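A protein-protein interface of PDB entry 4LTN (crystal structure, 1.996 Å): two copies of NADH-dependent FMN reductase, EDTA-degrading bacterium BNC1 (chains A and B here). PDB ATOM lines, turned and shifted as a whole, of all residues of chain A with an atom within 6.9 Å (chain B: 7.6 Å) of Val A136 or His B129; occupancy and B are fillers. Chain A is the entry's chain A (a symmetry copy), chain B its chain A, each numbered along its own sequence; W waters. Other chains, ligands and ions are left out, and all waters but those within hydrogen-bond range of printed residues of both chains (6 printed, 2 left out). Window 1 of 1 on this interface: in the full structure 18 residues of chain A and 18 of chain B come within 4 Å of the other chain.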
ATOM      1  N   LEU A 100     -13.565  28.337 -23.990  1.00  0.00           N
ATOM      2  CA  LEU A 100     -13.667  26.972 -23.488  1.00  0.00           C
ATOM      3  C   LEU A 100     -14.006  25.929 -24.552  1.00  0.00           C
ATOM      4  O   LEU A 100     -14.266  24.777 -24.222  1.00  0.00           O
ATOM      5  CB  LEU A 100     -14.672  26.891 -22.339  1.00  0.00           C
ATOM      6  CG  LEU A 100     -14.465  27.922 -21.233  1.00  0.00           C
ATOM      7  CD1 LEU A 100     -15.366  27.601 -20.043  1.00  0.00           C
ATOM      8  CD2 LEU A 100     -12.992  28.009 -20.823  1.00  0.00           C
ATOM      9  N   LYS A 103     -13.070  22.040 -24.442  1.00  0.00           N
ATOM     10  CA  LYS A 103     -12.673  21.666 -23.085  1.00  0.00           C
ATOM     11  C   LYS A 103     -13.753  20.977 -22.244  1.00  0.00           C
ATOM     12  O   LYS A 103     -14.938  21.270 -22.372  1.00  0.00           O
ATOM     13  CB  LYS A 103     -12.166  22.915 -22.351  1.00  0.00           C
ATOM     14  CG  LYS A 103     -11.142  23.713 -23.186  1.00  0.00           C
ATOM     15  CD  LYS A 103     -10.385  24.727 -22.354  1.00  0.00           C
ATOM     16  CE  LYS A 103      -9.571  25.660 -23.248  1.00  0.00           C
ATOM     17  NZ  LYS A 103      -8.758  24.910 -24.231  1.00  0.00           N
ATOM     18  N   ALA A 104     -13.321  20.058 -21.390  1.00  0.00           N
ATOM     19  CA  ALA A 104     -14.172  19.500 -20.346  1.00  0.00           C
ATOM     20  C   ALA A 104     -14.097  20.417 -19.132  1.00  0.00           C
ATOM     21  O   ALA A 104     -13.115  21.169 -18.981  1.00  0.00           O
ATOM     22  CB  ALA A 104     -13.700  18.096 -19.978  1.00  0.00           C
ATOM     23  N   ALA A 105     -15.108  20.373 -18.266  1.00  0.00           N
ATOM     24  CA  ALA A 105     -15.115  21.197 -17.051  1.00  0.00           C
ATOM     25  C   ALA A 105     -15.843  20.578 -15.864  1.00  0.00           C
ATOM     26  O   ALA A 105     -16.854  19.902 -16.038  1.00  0.00           O
ATOM     27  CB  ALA A 105     -15.681  22.593 -17.338  1.00  0.00           C
ATOM     28  N   LEU A 106     -15.339  20.850 -14.660  1.00  0.00           N
ATOM     29  CA  LEU A 106     -15.915  20.333 -13.417  1.00  0.00           C
ATOM     30  C   LEU A 106     -16.188  21.480 -12.456  1.00  0.00           C
ATOM     31  O   LEU A 106     -15.235  22.079 -11.929  1.00  0.00           O
ATOM     32  CB  LEU A 106     -14.930  19.358 -12.742  1.00  0.00           C
ATOM     33  CG  LEU A 106     -15.275  18.852 -11.339  1.00  0.00           C
ATOM     34  CD1 LEU A 106     -16.628  18.122 -11.343  1.00  0.00           C
ATOM     35  CD2 LEU A 106     -14.170  17.947 -10.787  1.00  0.00           C
ATOM     36  N   PRO A 107     -17.477  21.802 -12.226  1.00  0.00           N
ATOM     37  CA  PRO A 107     -17.832  22.880 -11.296  1.00  0.00           C
ATOM     38  C   PRO A 107     -17.866  22.395  -9.851  1.00  0.00           C
ATOM     39  O   PRO A 107     -18.559  21.418  -9.530  1.00  0.00           O
ATOM     40  CB  PRO A 107     -19.256  23.286 -11.736  1.00  0.00           C
ATOM     41  CG  PRO A 107     -19.558  22.487 -12.988  1.00  0.00           C
ATOM     42  CD  PRO A 107     -18.664  21.285 -12.934  1.00  0.00           C
ATOM     43  N   ASP A 121     -25.419  25.073 -10.755  1.00  0.00           N
ATOM     44  CA  ASP A 121     -26.159  24.718 -11.968  1.00  0.00           C
ATOM     45  C   ASP A 121     -26.978  25.872 -12.588  1.00  0.00           C
ATOM     46  O   ASP A 121     -27.095  25.969 -13.808  1.00  0.00           O
ATOM     47  CB  ASP A 121     -27.041  23.497 -11.712  1.00  0.00           C
ATOM     48  CG  ASP A 121     -26.251  22.191 -11.739  1.00  0.00           C
ATOM     49  OD1 ASP A 121     -25.049  22.211 -12.088  1.00  0.00           O
ATOM     50  OD2 ASP A 121     -26.846  21.136 -11.428  1.00  0.00           O
ATOM     51  N   ARG A 125     -22.926  27.328 -14.386  1.00  0.00           N
ATOM     52  CA  ARG A 125     -23.031  26.488 -15.581  1.00  0.00           C
ATOM     53  C   ARG A 125     -23.360  27.291 -16.840  1.00  0.00           C
ATOM     54  O   ARG A 125     -22.742  27.094 -17.876  1.00  0.00           O
ATOM     55  CB  ARG A 125     -24.048  25.354 -15.354  1.00  0.00           C
ATOM     56  CG  ARG A 125     -24.028  24.268 -16.433  1.00  0.00           C
ATOM     57  CD  ARG A 125     -24.975  23.100 -16.062  1.00  0.00           C
ATOM     58  NE  ARG A 125     -24.435  22.344 -14.941  1.00  0.00           N
ATOM     59  CZ  ARG A 125     -23.577  21.338 -15.067  1.00  0.00           C
ATOM     60  NH1 ARG A 125     -23.114  20.724 -13.983  1.00  0.00           N
ATOM     61  NH2 ARG A 125     -23.172  20.950 -16.275  1.00  0.00           N
ATOM     62  N   LEU A 128     -20.215  29.163 -18.152  1.00  0.00           N
ATOM     63  CA  LEU A 128     -19.297  28.283 -18.868  1.00  0.00           C
ATOM     64  C   LEU A 128     -19.818  27.997 -20.275  1.00  0.00           C
ATOM     65  O   LEU A 128     -19.054  27.930 -21.237  1.00  0.00           O
ATOM     66  CB  LEU A 128     -19.109  26.975 -18.103  1.00  0.00           C
ATOM     67  CG  LEU A 128     -18.521  27.114 -16.701  1.00  0.00           C
ATOM     68  CD1 LEU A 128     -18.393  25.752 -16.031  1.00  0.00           C
ATOM     69  CD2 LEU A 128     -17.154  27.817 -16.793  1.00  0.00           C
ATOM     70  N   HIS A 129     -21.131  27.814 -20.400  1.00  0.00           N
ATOM     71  CA  HIS A 129     -21.696  27.570 -21.724  1.00  0.00           C
ATOM     72  C   HIS A 129     -21.693  28.775 -22.659  1.00  0.00           C
ATOM     73  O   HIS A 129     -21.705  28.617 -23.870  1.00  0.00           O
ATOM     74  CB  HIS A 129     -23.071  26.913 -21.618  1.00  0.00           C
ATOM     75  CG  HIS A 129     -22.975  25.448 -21.378  1.00  0.00           C
ATOM     76  ND1 HIS A 129     -22.705  24.553 -22.390  1.00  0.00           N
ATOM     77  CD2 HIS A 129     -23.041  24.721 -20.238  1.00  0.00           C
ATOM     78  CE1 HIS A 129     -22.621  23.334 -21.885  1.00  0.00           C
ATOM     79  NE2 HIS A 129     -22.829  23.409 -20.581  1.00  0.00           N
ATOM     80  N   VAL A 133     -17.926  25.908 -24.113  1.00  0.00           N
ATOM     81  CA  VAL A 133     -17.390  24.752 -23.397  1.00  0.00           C
ATOM     82  C   VAL A 133     -17.893  23.432 -24.012  1.00  0.00           C
ATOM     83  O   VAL A 133     -19.040  23.343 -24.457  1.00  0.00           O
ATOM     84  CB  VAL A 133     -17.740  24.830 -21.888  1.00  0.00           C
ATOM     85  CG1 VAL A 133     -19.242  24.581 -21.656  1.00  0.00           C
ATOM     86  CG2 VAL A 133     -16.900  23.852 -21.076  1.00  0.00           C
ATOM     87  N   ARG A 134     -17.038  22.411 -24.047  1.00  0.00           N
ATOM     88  CA  ARG A 134     -17.426  21.165 -24.712  1.00  0.00           C
ATOM     89  C   ARG A 134     -18.307  20.254 -23.846  1.00  0.00           C
ATOM     90  O   ARG A 134     -19.356  19.740 -24.315  1.00  0.00           O
ATOM     91  CB  ARG A 134     -16.206  20.387 -25.227  1.00  0.00           C
ATOM     92  CG  ARG A 134     -16.581  19.077 -25.953  1.00  0.00           C
ATOM     93  CD  ARG A 134     -15.340  18.346 -26.484  1.00  0.00           C
ATOM     94  NE  ARG A 134     -14.424  17.983 -25.405  1.00  0.00           N
ATOM     95  CZ  ARG A 134     -14.591  16.925 -24.625  1.00  0.00           C
ATOM     96  NH1 ARG A 134     -15.653  16.127 -24.805  1.00  0.00           N
ATOM     97  NH2 ARG A 134     -13.709  16.671 -23.658  1.00  0.00           N
ATOM     98  N   HIS A 135     -17.884  20.059 -22.598  1.00  0.00           N
ATOM     99  CA  HIS A 135     -18.560  19.120 -21.704  1.00  0.00           C
ATOM    100  C   HIS A 135     -18.372  19.542 -20.268  1.00  0.00           C
ATOM    101  O   HIS A 135     -17.250  19.463 -19.740  1.00  0.00           O
ATOM    102  CB  HIS A 135     -17.985  17.703 -21.890  1.00  0.00           C
ATOM    103  CG  HIS A 135     -18.766  16.626 -21.189  1.00  0.00           C
ATOM    104  ND1 HIS A 135     -18.467  15.285 -21.326  1.00  0.00           N
ATOM    105  CD2 HIS A 135     -19.846  16.688 -20.370  1.00  0.00           C
ATOM    106  CE1 HIS A 135     -19.321  14.566 -20.612  1.00  0.00           C
ATOM    107  NE2 HIS A 135     -20.169  15.392 -20.023  1.00  0.00           N
ATOM    108  N   VAL A 136     -19.451  19.993 -19.630  1.00  0.00           N
ATOM    109  CA  VAL A 136     -19.416  20.278 -18.198  1.00  0.00           C
ATOM    110  C   VAL A 136     -20.102  19.135 -17.475  1.00  0.00           C
ATOM    111  O   VAL A 136     -21.301  18.909 -17.686  1.00  0.00           O
ATOM    112  CB  VAL A 136     -20.170  21.571 -17.842  1.00  0.00           C
ATOM    113  CG1 VAL A 136     -19.983  21.913 -16.357  1.00  0.00           C
ATOM    114  CG2 VAL A 136     -19.753  22.720 -18.758  1.00  0.00           C
ATOM    115  N   VAL A 137     -19.366  18.392 -16.648  1.00  0.00           N
ATOM    116  CA  VAL A 137     -19.979  17.240 -15.973  1.00  0.00           C
ATOM    117  C   VAL A 137     -20.778  17.728 -14.778  1.00  0.00           C
ATOM    118  O   VAL A 137     -20.983  18.930 -14.620  1.00  0.00           O
ATOM    119  CB  VAL A 137     -18.932  16.195 -15.536  1.00  0.00           C
ATOM    120  CG1 VAL A 137     -18.151  15.708 -16.752  1.00  0.00           C
ATOM    121  CG2 VAL A 137     -17.974  16.784 -14.490  1.00  0.00           C
ATOM    122  N   GLN A 138     -21.222  16.813 -13.926  1.00  0.00           N
ATOM    123  CA  GLN A 138     -22.063  17.213 -12.809  1.00  0.00           C
ATOM    124  C   GLN A 138     -21.338  18.169 -11.868  1.00  0.00           C
ATOM    125  O   GLN A 138     -20.113  18.102 -11.716  1.00  0.00           O
ATOM    126  CB  GLN A 138     -22.570  16.007 -12.020  1.00  0.00           C
ATOM    127  CG  GLN A 138     -21.477  15.201 -11.320  1.00  0.00           C
ATOM    128  CD  GLN A 138     -21.148  13.913 -12.062  1.00  0.00           C
ATOM    129  OE1 GLN A 138     -21.093  13.886 -13.292  1.00  0.00           O
ATOM    130  NE2 GLN A 138     -20.928  12.841 -11.313  1.00  0.00           N
ATOM    131  N   SER A 139     -22.106  19.050 -11.238  1.00  0.00           N
ATOM    132  CA  SER A 139     -21.566  19.949 -10.216  1.00  0.00           C
ATOM    133  C   SER A 139     -21.386  19.202  -8.915  1.00  0.00           C
ATOM    134  O   SER A 139     -22.115  18.252  -8.640  1.00  0.00           O
ATOM    135  CB  SER A 139     -22.545  21.095  -9.968  1.00  0.00           C
ATOM    136  OG  SER A 139     -22.726  21.851 -11.148  1.00  0.00           O
ATOM    137  N   HIS A 170     -15.805  11.317 -13.300  1.00  0.00           N
ATOM    138  CA  HIS A 170     -16.488  11.598 -14.551  1.00  0.00           C
ATOM    139  C   HIS A 170     -15.727  12.676 -15.326  1.00  0.00           C
ATOM    140  O   HIS A 170     -15.503  12.556 -16.529  1.00  0.00           O
ATOM    141  CB  HIS A 170     -17.932  12.019 -14.324  1.00  0.00           C
ATOM    142  CG  HIS A 170     -18.716  12.119 -15.593  1.00  0.00           C
ATOM    143  ND1 HIS A 170     -19.979  12.675 -15.648  1.00  0.00           N
ATOM    144  CD2 HIS A 170     -18.413  11.741 -16.857  1.00  0.00           C
ATOM    145  CE1 HIS A 170     -20.417  12.633 -16.896  1.00  0.00           C
ATOM    146  NE2 HIS A 170     -19.491  12.068 -17.650  1.00  0.00           N
ATOM    147  N   SER A 174     -14.140  12.304 -19.037  1.00  0.00           N
ATOM    148  CA  SER A 174     -14.684  13.142 -20.101  1.00  0.00           C
ATOM    149  C   SER A 174     -13.579  13.823 -20.922  1.00  0.00           C
ATOM    150  O   SER A 174     -13.845  14.357 -22.000  1.00  0.00           O
ATOM    151  CB  SER A 174     -15.630  14.199 -19.522  1.00  0.00           C
ATOM    152  OG  SER A 174     -14.880  15.223 -18.871  1.00  0.00           O
ATOM    153  N   GLN B  97     -36.046   9.549 -10.754  1.00  0.00           N
ATOM    154  CA  GLN B  97     -35.205  10.613 -10.206  1.00  0.00           C
ATOM    155  C   GLN B  97     -33.901  10.799 -10.984  1.00  0.00           C
ATOM    156  O   GLN B  97     -33.476  11.928 -11.250  1.00  0.00           O
ATOM    157  CB  GLN B  97     -34.888  10.356  -8.728  1.00  0.00           C
ATOM    158  CG  GLN B  97     -34.074  11.470  -8.098  1.00  0.00           C
ATOM    159  CD  GLN B  97     -33.850  11.280  -6.609  1.00  0.00           C
ATOM    160  OE1 GLN B  97     -34.335  10.323  -6.016  1.00  0.00           O
ATOM    161  NE2 GLN B  97     -33.114  12.200  -5.999  1.00  0.00           N
ATOM    162  N   PHE B  98     -33.257   9.698 -11.342  1.00  0.00           N
ATOM    163  CA  PHE B  98     -32.001   9.799 -12.083  1.00  0.00           C
ATOM    164  C   PHE B  98     -32.142   9.255 -13.500  1.00  0.00           C
ATOM    165  O   PHE B  98     -31.246   8.601 -14.028  1.00  0.00           O
ATOM    166  CB  PHE B  98     -30.862   9.137 -11.309  1.00  0.00           C
ATOM    167  CG  PHE B  98     -30.542   9.838 -10.017  1.00  0.00           C
ATOM    168  CD1 PHE B  98     -29.985  11.107 -10.026  1.00  0.00           C
ATOM    169  CD2 PHE B  98     -30.819   9.241  -8.797  1.00  0.00           C
ATOM    170  CE1 PHE B  98     -29.696  11.767  -8.839  1.00  0.00           C
ATOM    171  CE2 PHE B  98     -30.530   9.893  -7.609  1.00  0.00           C
ATOM    172  CZ  PHE B  98     -29.969  11.159  -7.631  1.00  0.00           C
ATOM    173  N   LEU B 100     -31.821  10.271 -16.428  1.00  0.00           N
ATOM    174  CA  LEU B 100     -30.948  10.599 -17.550  1.00  0.00           C
ATOM    175  C   LEU B 100     -29.499  10.146 -17.377  1.00  0.00           C
ATOM    176  O   LEU B 100     -28.646  10.498 -18.183  1.00  0.00           O
ATOM    177  CB  LEU B 100     -30.996  12.096 -17.853  1.00  0.00           C
ATOM    178  CG  LEU B 100     -32.399  12.677 -17.999  1.00  0.00           C
ATOM    179  CD1 LEU B 100     -32.322  14.107 -18.527  1.00  0.00           C
ATOM    180  CD2 LEU B 100     -33.278  11.790 -18.885  1.00  0.00           C
ATOM    181  N   LEU B 124     -33.865  25.157 -18.656  1.00  0.00           N
ATOM    182  CA  LEU B 124     -33.962  23.719 -18.935  1.00  0.00           C
ATOM    183  C   LEU B 124     -32.717  22.927 -18.518  1.00  0.00           C
ATOM    184  O   LEU B 124     -32.805  21.788 -18.045  1.00  0.00           O
ATOM    185  CB  LEU B 124     -34.212  23.495 -20.428  1.00  0.00           C
ATOM    186  CG  LEU B 124     -34.452  22.038 -20.856  1.00  0.00           C
ATOM    187  CD1 LEU B 124     -35.580  21.403 -20.024  1.00  0.00           C
ATOM    188  CD2 LEU B 124     -34.751  21.953 -22.361  1.00  0.00           C
ATOM    189  N   ARG B 125     -31.548  23.520 -18.735  1.00  0.00           N
ATOM    190  CA  ARG B 125     -30.295  22.812 -18.463  1.00  0.00           C
ATOM    191  C   ARG B 125     -30.197  22.321 -17.017  1.00  0.00           C
ATOM    192  O   ARG B 125     -29.822  21.182 -16.778  1.00  0.00           O
ATOM    193  CB  ARG B 125     -29.088  23.691 -18.840  1.00  0.00           C
ATOM    194  CG  ARG B 125     -27.750  22.947 -18.853  1.00  0.00           C
ATOM    195  CD  ARG B 125     -26.613  23.860 -19.377  1.00  0.00           C
ATOM    196  NE  ARG B 125     -26.773  24.104 -20.802  1.00  0.00           N
ATOM    197  CZ  ARG B 125     -26.292  23.307 -21.751  1.00  0.00           C
ATOM    198  NH1 ARG B 125     -26.513  23.595 -23.030  1.00  0.00           N
ATOM    199  NH2 ARG B 125     -25.600  22.218 -21.424  1.00  0.00           N
ATOM    200  N   PRO B 126     -30.545  23.172 -16.036  1.00  0.00           N
ATOM    201  CA  PRO B 126     -30.481  22.711 -14.640  1.00  0.00           C
ATOM    202  C   PRO B 126     -31.454  21.569 -14.339  1.00  0.00           C
ATOM    203  O   PRO B 126     -31.161  20.717 -13.502  1.00  0.00           O
ATOM    204  CB  PRO B 126     -30.862  23.959 -13.830  1.00  0.00           C
ATOM    205  CG  PRO B 126     -30.537  25.100 -14.735  1.00  0.00           C
ATOM    206  CD  PRO B 126     -30.846  24.612 -16.127  1.00  0.00           C
ATOM    207  N   VAL B 127     -32.595  21.539 -15.017  1.00  0.00           N
ATOM    208  CA  VAL B 127     -33.550  20.460 -14.799  1.00  0.00           C
ATOM    209  C   VAL B 127     -32.982  19.133 -15.303  1.00  0.00           C
ATOM    210  O   VAL B 127     -33.098  18.110 -14.640  1.00  0.00           O
ATOM    211  CB  VAL B 127     -34.900  20.781 -15.477  1.00  0.00           C
ATOM    212  CG1 VAL B 127     -35.805  19.554 -15.513  1.00  0.00           C
ATOM    213  CG2 VAL B 127     -35.576  21.951 -14.763  1.00  0.00           C
ATOM    214  N   LEU B 128     -32.371  19.142 -16.484  1.00  0.00           N
ATOM    215  CA  LEU B 128     -31.741  17.937 -17.012  1.00  0.00           C
ATOM    216  C   LEU B 128     -30.645  17.448 -16.067  1.00  0.00           C
ATOM    217  O   LEU B 128     -30.468  16.249 -15.860  1.00  0.00           O
ATOM    218  CB  LEU B 128     -31.156  18.204 -18.397  1.00  0.00           C
ATOM    219  CG  LEU B 128     -32.164  18.630 -19.462  1.00  0.00           C
ATOM    220  CD1 LEU B 128     -31.468  18.884 -20.793  1.00  0.00           C
ATOM    221  CD2 LEU B 128     -33.245  17.543 -19.600  1.00  0.00           C
ATOM    222  N   HIS B 129     -29.890  18.383 -15.493  1.00  0.00           N
ATOM    223  CA  HIS B 129     -28.847  17.984 -14.553  1.00  0.00           C
ATOM    224  C   HIS B 129     -29.353  17.456 -13.214  1.00  0.00           C
ATOM    225  O   HIS B 129     -28.662  16.700 -12.548  1.00  0.00           O
ATOM    226  CB  HIS B 129     -27.805  19.089 -14.391  1.00  0.00           C
ATOM    227  CG  HIS B 129     -26.816  19.092 -15.503  1.00  0.00           C
ATOM    228  ND1 HIS B 129     -25.763  18.205 -15.553  1.00  0.00           N
ATOM    229  CD2 HIS B 129     -26.752  19.821 -16.642  1.00  0.00           C
ATOM    230  CE1 HIS B 129     -25.084  18.397 -16.671  1.00  0.00           C
ATOM    231  NE2 HIS B 129     -25.660  19.378 -17.346  1.00  0.00           N
ATOM    232  N   SER B 130     -30.580  17.803 -12.839  1.00  0.00           N
ATOM    233  CA  SER B 130     -31.166  17.207 -11.640  1.00  0.00           C
ATOM    234  C   SER B 130     -31.425  15.711 -11.854  1.00  0.00           C
ATOM    235  O   SER B 130     -31.635  14.975 -10.903  1.00  0.00           O
ATOM    236  CB  SER B 130     -32.453  17.934 -11.227  1.00  0.00           C
ATOM    237  OG  SER B 130     -33.595  17.379 -11.868  1.00  0.00           O
ATOM    238  N   MET B 131     -31.375  15.258 -13.103  1.00  0.00           N
ATOM    239  CA  MET B 131     -31.729  13.867 -13.437  1.00  0.00           C
ATOM    240  C   MET B 131     -30.509  12.994 -13.779  1.00  0.00           C
ATOM    241  O   MET B 131     -30.646  11.898 -14.338  1.00  0.00           O
ATOM    242  CB  MET B 131     -32.778  13.821 -14.556  1.00  0.00           C
ATOM    243  CG  MET B 131     -34.206  13.902 -14.037  1.00  0.00           C
ATOM    244  SD  MET B 131     -35.574  13.814 -15.413  1.00  0.00           S
ATOM    245  CE  MET B 131     -35.255  15.596 -15.965  1.00  0.00           C
ATOM    246  N   GLY B 132     -29.319  13.479 -13.429  1.00  0.00           N
ATOM    247  CA  GLY B 132     -28.107  12.683 -13.555  1.00  0.00           C
ATOM    248  C   GLY B 132     -27.592  12.563 -14.977  1.00  0.00           C
ATOM    249  O   GLY B 132     -26.790  11.674 -15.271  1.00  0.00           O
ATOM    250  N   VAL B 133     -28.033  13.472 -15.844  1.00  0.00           N
ATOM    251  CA  VAL B 133     -27.692  13.446 -17.265  1.00  0.00           C
ATOM    252  C   VAL B 133     -26.166  13.389 -17.472  1.00  0.00           C
ATOM    253  O   VAL B 133     -25.407  13.999 -16.716  1.00  0.00           O
ATOM    254  CB  VAL B 133     -28.306  14.666 -18.001  1.00  0.00           C
ATOM    255  CG1 VAL B 133     -27.586  15.969 -17.604  1.00  0.00           C
ATOM    256  CG2 VAL B 133     -28.275  14.472 -19.512  1.00  0.00           C
ATOM    257  N   ARG B 134     -25.716  12.652 -18.485  1.00  0.00           N
ATOM    258  CA  ARG B 134     -24.273  12.477 -18.668  1.00  0.00           C
ATOM    259  C   ARG B 134     -23.594  13.659 -19.371  1.00  0.00           C
ATOM    260  O   ARG B 134     -22.534  14.159 -18.912  1.00  0.00           O
ATOM    261  CB  ARG B 134     -23.942  11.167 -19.398  1.00  0.00           C
ATOM    262  CG  ARG B 134     -22.427  10.941 -19.587  1.00  0.00           C
ATOM    263  CD  ARG B 134     -22.134   9.606 -20.289  1.00  0.00           C
ATOM    264  NE  ARG B 134     -22.739   9.550 -21.617  1.00  0.00           N
ATOM    265  CZ  ARG B 134     -22.207  10.116 -22.691  1.00  0.00           C
ATOM    266  NH1 ARG B 134     -21.053  10.792 -22.583  1.00  0.00           N
ATOM    267  NH2 ARG B 134     -22.830  10.022 -23.865  1.00  0.00           N
ATOM    268  N   HIS B 135     -24.200  14.101 -20.472  1.00  0.00           N
ATOM    269  CA  HIS B 135     -23.599  15.141 -21.306  1.00  0.00           C
ATOM    270  C   HIS B 135     -24.674  15.914 -22.030  1.00  0.00           C
ATOM    271  O   HIS B 135     -25.330  15.366 -22.932  1.00  0.00           O
ATOM    272  CB  HIS B 135     -22.651  14.508 -22.342  1.00  0.00           C
ATOM    273  CG  HIS B 135     -21.808  15.502 -23.094  1.00  0.00           C
ATOM    274  ND1 HIS B 135     -20.826  15.119 -23.985  1.00  0.00           N
ATOM    275  CD2 HIS B 135     -21.782  16.858 -23.067  1.00  0.00           C
ATOM    276  CE1 HIS B 135     -20.238  16.195 -24.485  1.00  0.00           C
ATOM    277  NE2 HIS B 135     -20.797  17.263 -23.945  1.00  0.00           N
ATOM    278  N   VAL B 136     -24.865  17.174 -21.647  1.00  0.00           N
ATOM    279  CA  VAL B 136     -25.768  18.058 -22.383  1.00  0.00           C
ATOM    280  C   VAL B 136     -24.924  18.988 -23.233  1.00  0.00           C
ATOM    281  O   VAL B 136     -24.144  19.779 -22.685  1.00  0.00           O
ATOM    282  CB  VAL B 136     -26.622  18.930 -21.447  1.00  0.00           C
ATOM    283  CG1 VAL B 136     -27.657  19.729 -22.252  1.00  0.00           C
ATOM    284  CG2 VAL B 136     -27.267  18.088 -20.348  1.00  0.00           C
ATOM    285  N   VAL B 137     -25.039  18.895 -24.558  1.00  0.00           N
ATOM    286  CA  VAL B 137     -24.197  19.739 -25.417  1.00  0.00           C
ATOM    287  C   VAL B 137     -24.796  21.132 -25.490  1.00  0.00           C
ATOM    288  O   VAL B 137     -25.718  21.450 -24.743  1.00  0.00           O
ATOM    289  CB  VAL B 137     -24.028  19.145 -26.831  1.00  0.00           C
ATOM    290  CG1 VAL B 137     -23.414  17.753 -26.735  1.00  0.00           C
ATOM    291  CG2 VAL B 137     -25.377  19.083 -27.563  1.00  0.00           C
ATOM    292  N   GLY B 185     -22.734  10.488 -14.745  1.00  0.00           N
ATOM    293  CA  GLY B 185     -23.644  11.588 -14.473  1.00  0.00           C
ATOM    294  C   GLY B 185     -24.457  11.355 -13.213  1.00  0.00           C
ATOM    295  O   GLY B 185     -24.919  12.296 -12.583  1.00  0.00           O
ATOM    296  N   PRO B 187     -24.865  10.630  -9.352  1.00  0.00           N
ATOM    297  CA  PRO B 187     -23.994  10.938  -8.208  1.00  0.00           C
ATOM    298  C   PRO B 187     -23.537   9.688  -7.445  1.00  0.00           C
ATOM    299  O   PRO B 187     -22.533   9.747  -6.737  1.00  0.00           O
ATOM    300  CB  PRO B 187     -24.887  11.814  -7.317  1.00  0.00           C
ATOM    301  CG  PRO B 187     -26.279  11.412  -7.676  1.00  0.00           C
ATOM    302  CD  PRO B 187     -26.236  11.132  -9.148  1.00  0.00           C
HETATM  303  O   HOH W   1     -29.617  20.786 -11.193  1.00  0.00           O
HETATM  304  O   HOH W   2     -21.730  20.276 -21.278  1.00  0.00           O
HETATM  305  O   HOH W   3     -19.191  11.137 -20.244  1.00  0.00           O
HETATM  306  O   HOH W   4     -21.086  10.045 -12.507  1.00  0.00           O
HETATM  307  O   HOH W   5     -22.659  15.244 -16.286  1.00  0.00           O
HETATM  308  O   HOH W   6     -23.360  17.934 -19.377  1.00  0.00           O
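NH2 of Arg B125 lies within hydrogen-bond range of NE2 of His A129, 3.1 Å away.
NE2 of His B129 is in hydrogen-bond range of NH2 of Arg A125 (3.1 Å).
A ring nitrogen (NE2) of His B135 is in hydrogen-bond range of the backbone carbonyl oxygen of Arg A134, at 2.9 Å.
O of Arg B134 is in hydrogen-bond range of NE2 of His A135, 2.9 Å away.
NH1 of Arg A125 sits at hydrogen-bond distance from O of Val A137 (2.9 Å).
O of Val A136 sits at hydrogen-bond distance from NH2 of Arg A125.
The guanidinium group (NH1) of Arg B125 is in hydrogen-bond range of the backbone carbonyl oxygen (O) of Val B137 (2.9 Å).
The side-chain amide oxygen of Gln A138 sits at hydrogen-bond distance from a ring nitrogen (ND1) of His A170, at 2.9 Å.
The side-chain hydroxyl (OG) of Ser A139 is in hydrogen-bond range of the guanidinium group (NH1) of Arg A125 (3.1 Å).
Asp A121 touches Pro B126.
Asp A121 touches His B129.
Arg B125 touches Arg A125.
O of Val B136 touches CE1 of His A129, at 3.9 Å.
His A135 touches His B135 (CD2 to CD2, 3.3 Å).
Val A136 touches His B129 (O to CE1, 3.95 Å).
Gly B185 touches Gln A138 (CA to OE1, 3.6 Å).
CE1 of His A170 touches O of Arg B134, at 3.3 Å.
Gly B185 touches His A170 (N to ND1, 3.6 Å).
Of the printed residues of chain B, Asp A121 touches Pro B126 and His B129.
Printed residues of chain B within 4 Å of His A129: Arg B125 (3.1 Å) and Val B136 (3.9 Å).
Val A133 touches none of the printed residues of chain B.
Of chain B, only His B129 comes within 4 Å of Val A136.
Printed residues of chain B within 4 Å of His A170: Arg B134 (3.3 Å) and Gly B185 (3.6 Å).
Leu B100 touches none of the printed residues of chain A.
Printed residues of chain A within 4 Å of Gly B185: Gln A138 (3.6 Å) and His A170 (3.6 Å).
The nearest residue of chain A that does not touch His B129 is Val A137 (4.6 Å).
The nearest printed residue of chain B that does not touch His A170 is Val B133 (5.2 Å).
Hydrophobic or aromatic side chains of chain A within 4 Å of the printed part of chain B: His A129, His A135 and His A170.
Of the 19 printed residues of chain B, 7 touch a printed residue of chain A.
Hydrophobic or aromatic side chains of chain B within 4 Å of the printed part of chain A: Pro B126, His B129 and His B135.
Arg A125 touches His B129, and with the chains exchanged His A129 touches Arg B125.
His A129 touches Val B136, and with the chains exchanged Val A136 touches His B129.
Arg A134 touches His B135, and with the chains exchanged His A135 touches Arg B134.
His B135 touches its own counterpart, His A135.
Of the 13 pairs that touch across the chains among the printed residues, 8 have their exchanged pair printed and touching as well.
Water W1 lies within hydrogen-bond range of O of Pro B126 and OD2 of Asp A121.
Water W2 lies within hydrogen-bond range of the backbone NH (N) of Val A136 (2.8 Å), the backbone carbonyl oxygen (O) of Val B136 (2.8 Å) and a ring nitrogen (NE2) of His A129 (3.4 Å).
Water W5 lies within hydrogen-bond range of O of Arg B134 (2.8 Å), O of Val B133 (3.0 Å) and N of Gln A138 (3.2 Å).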
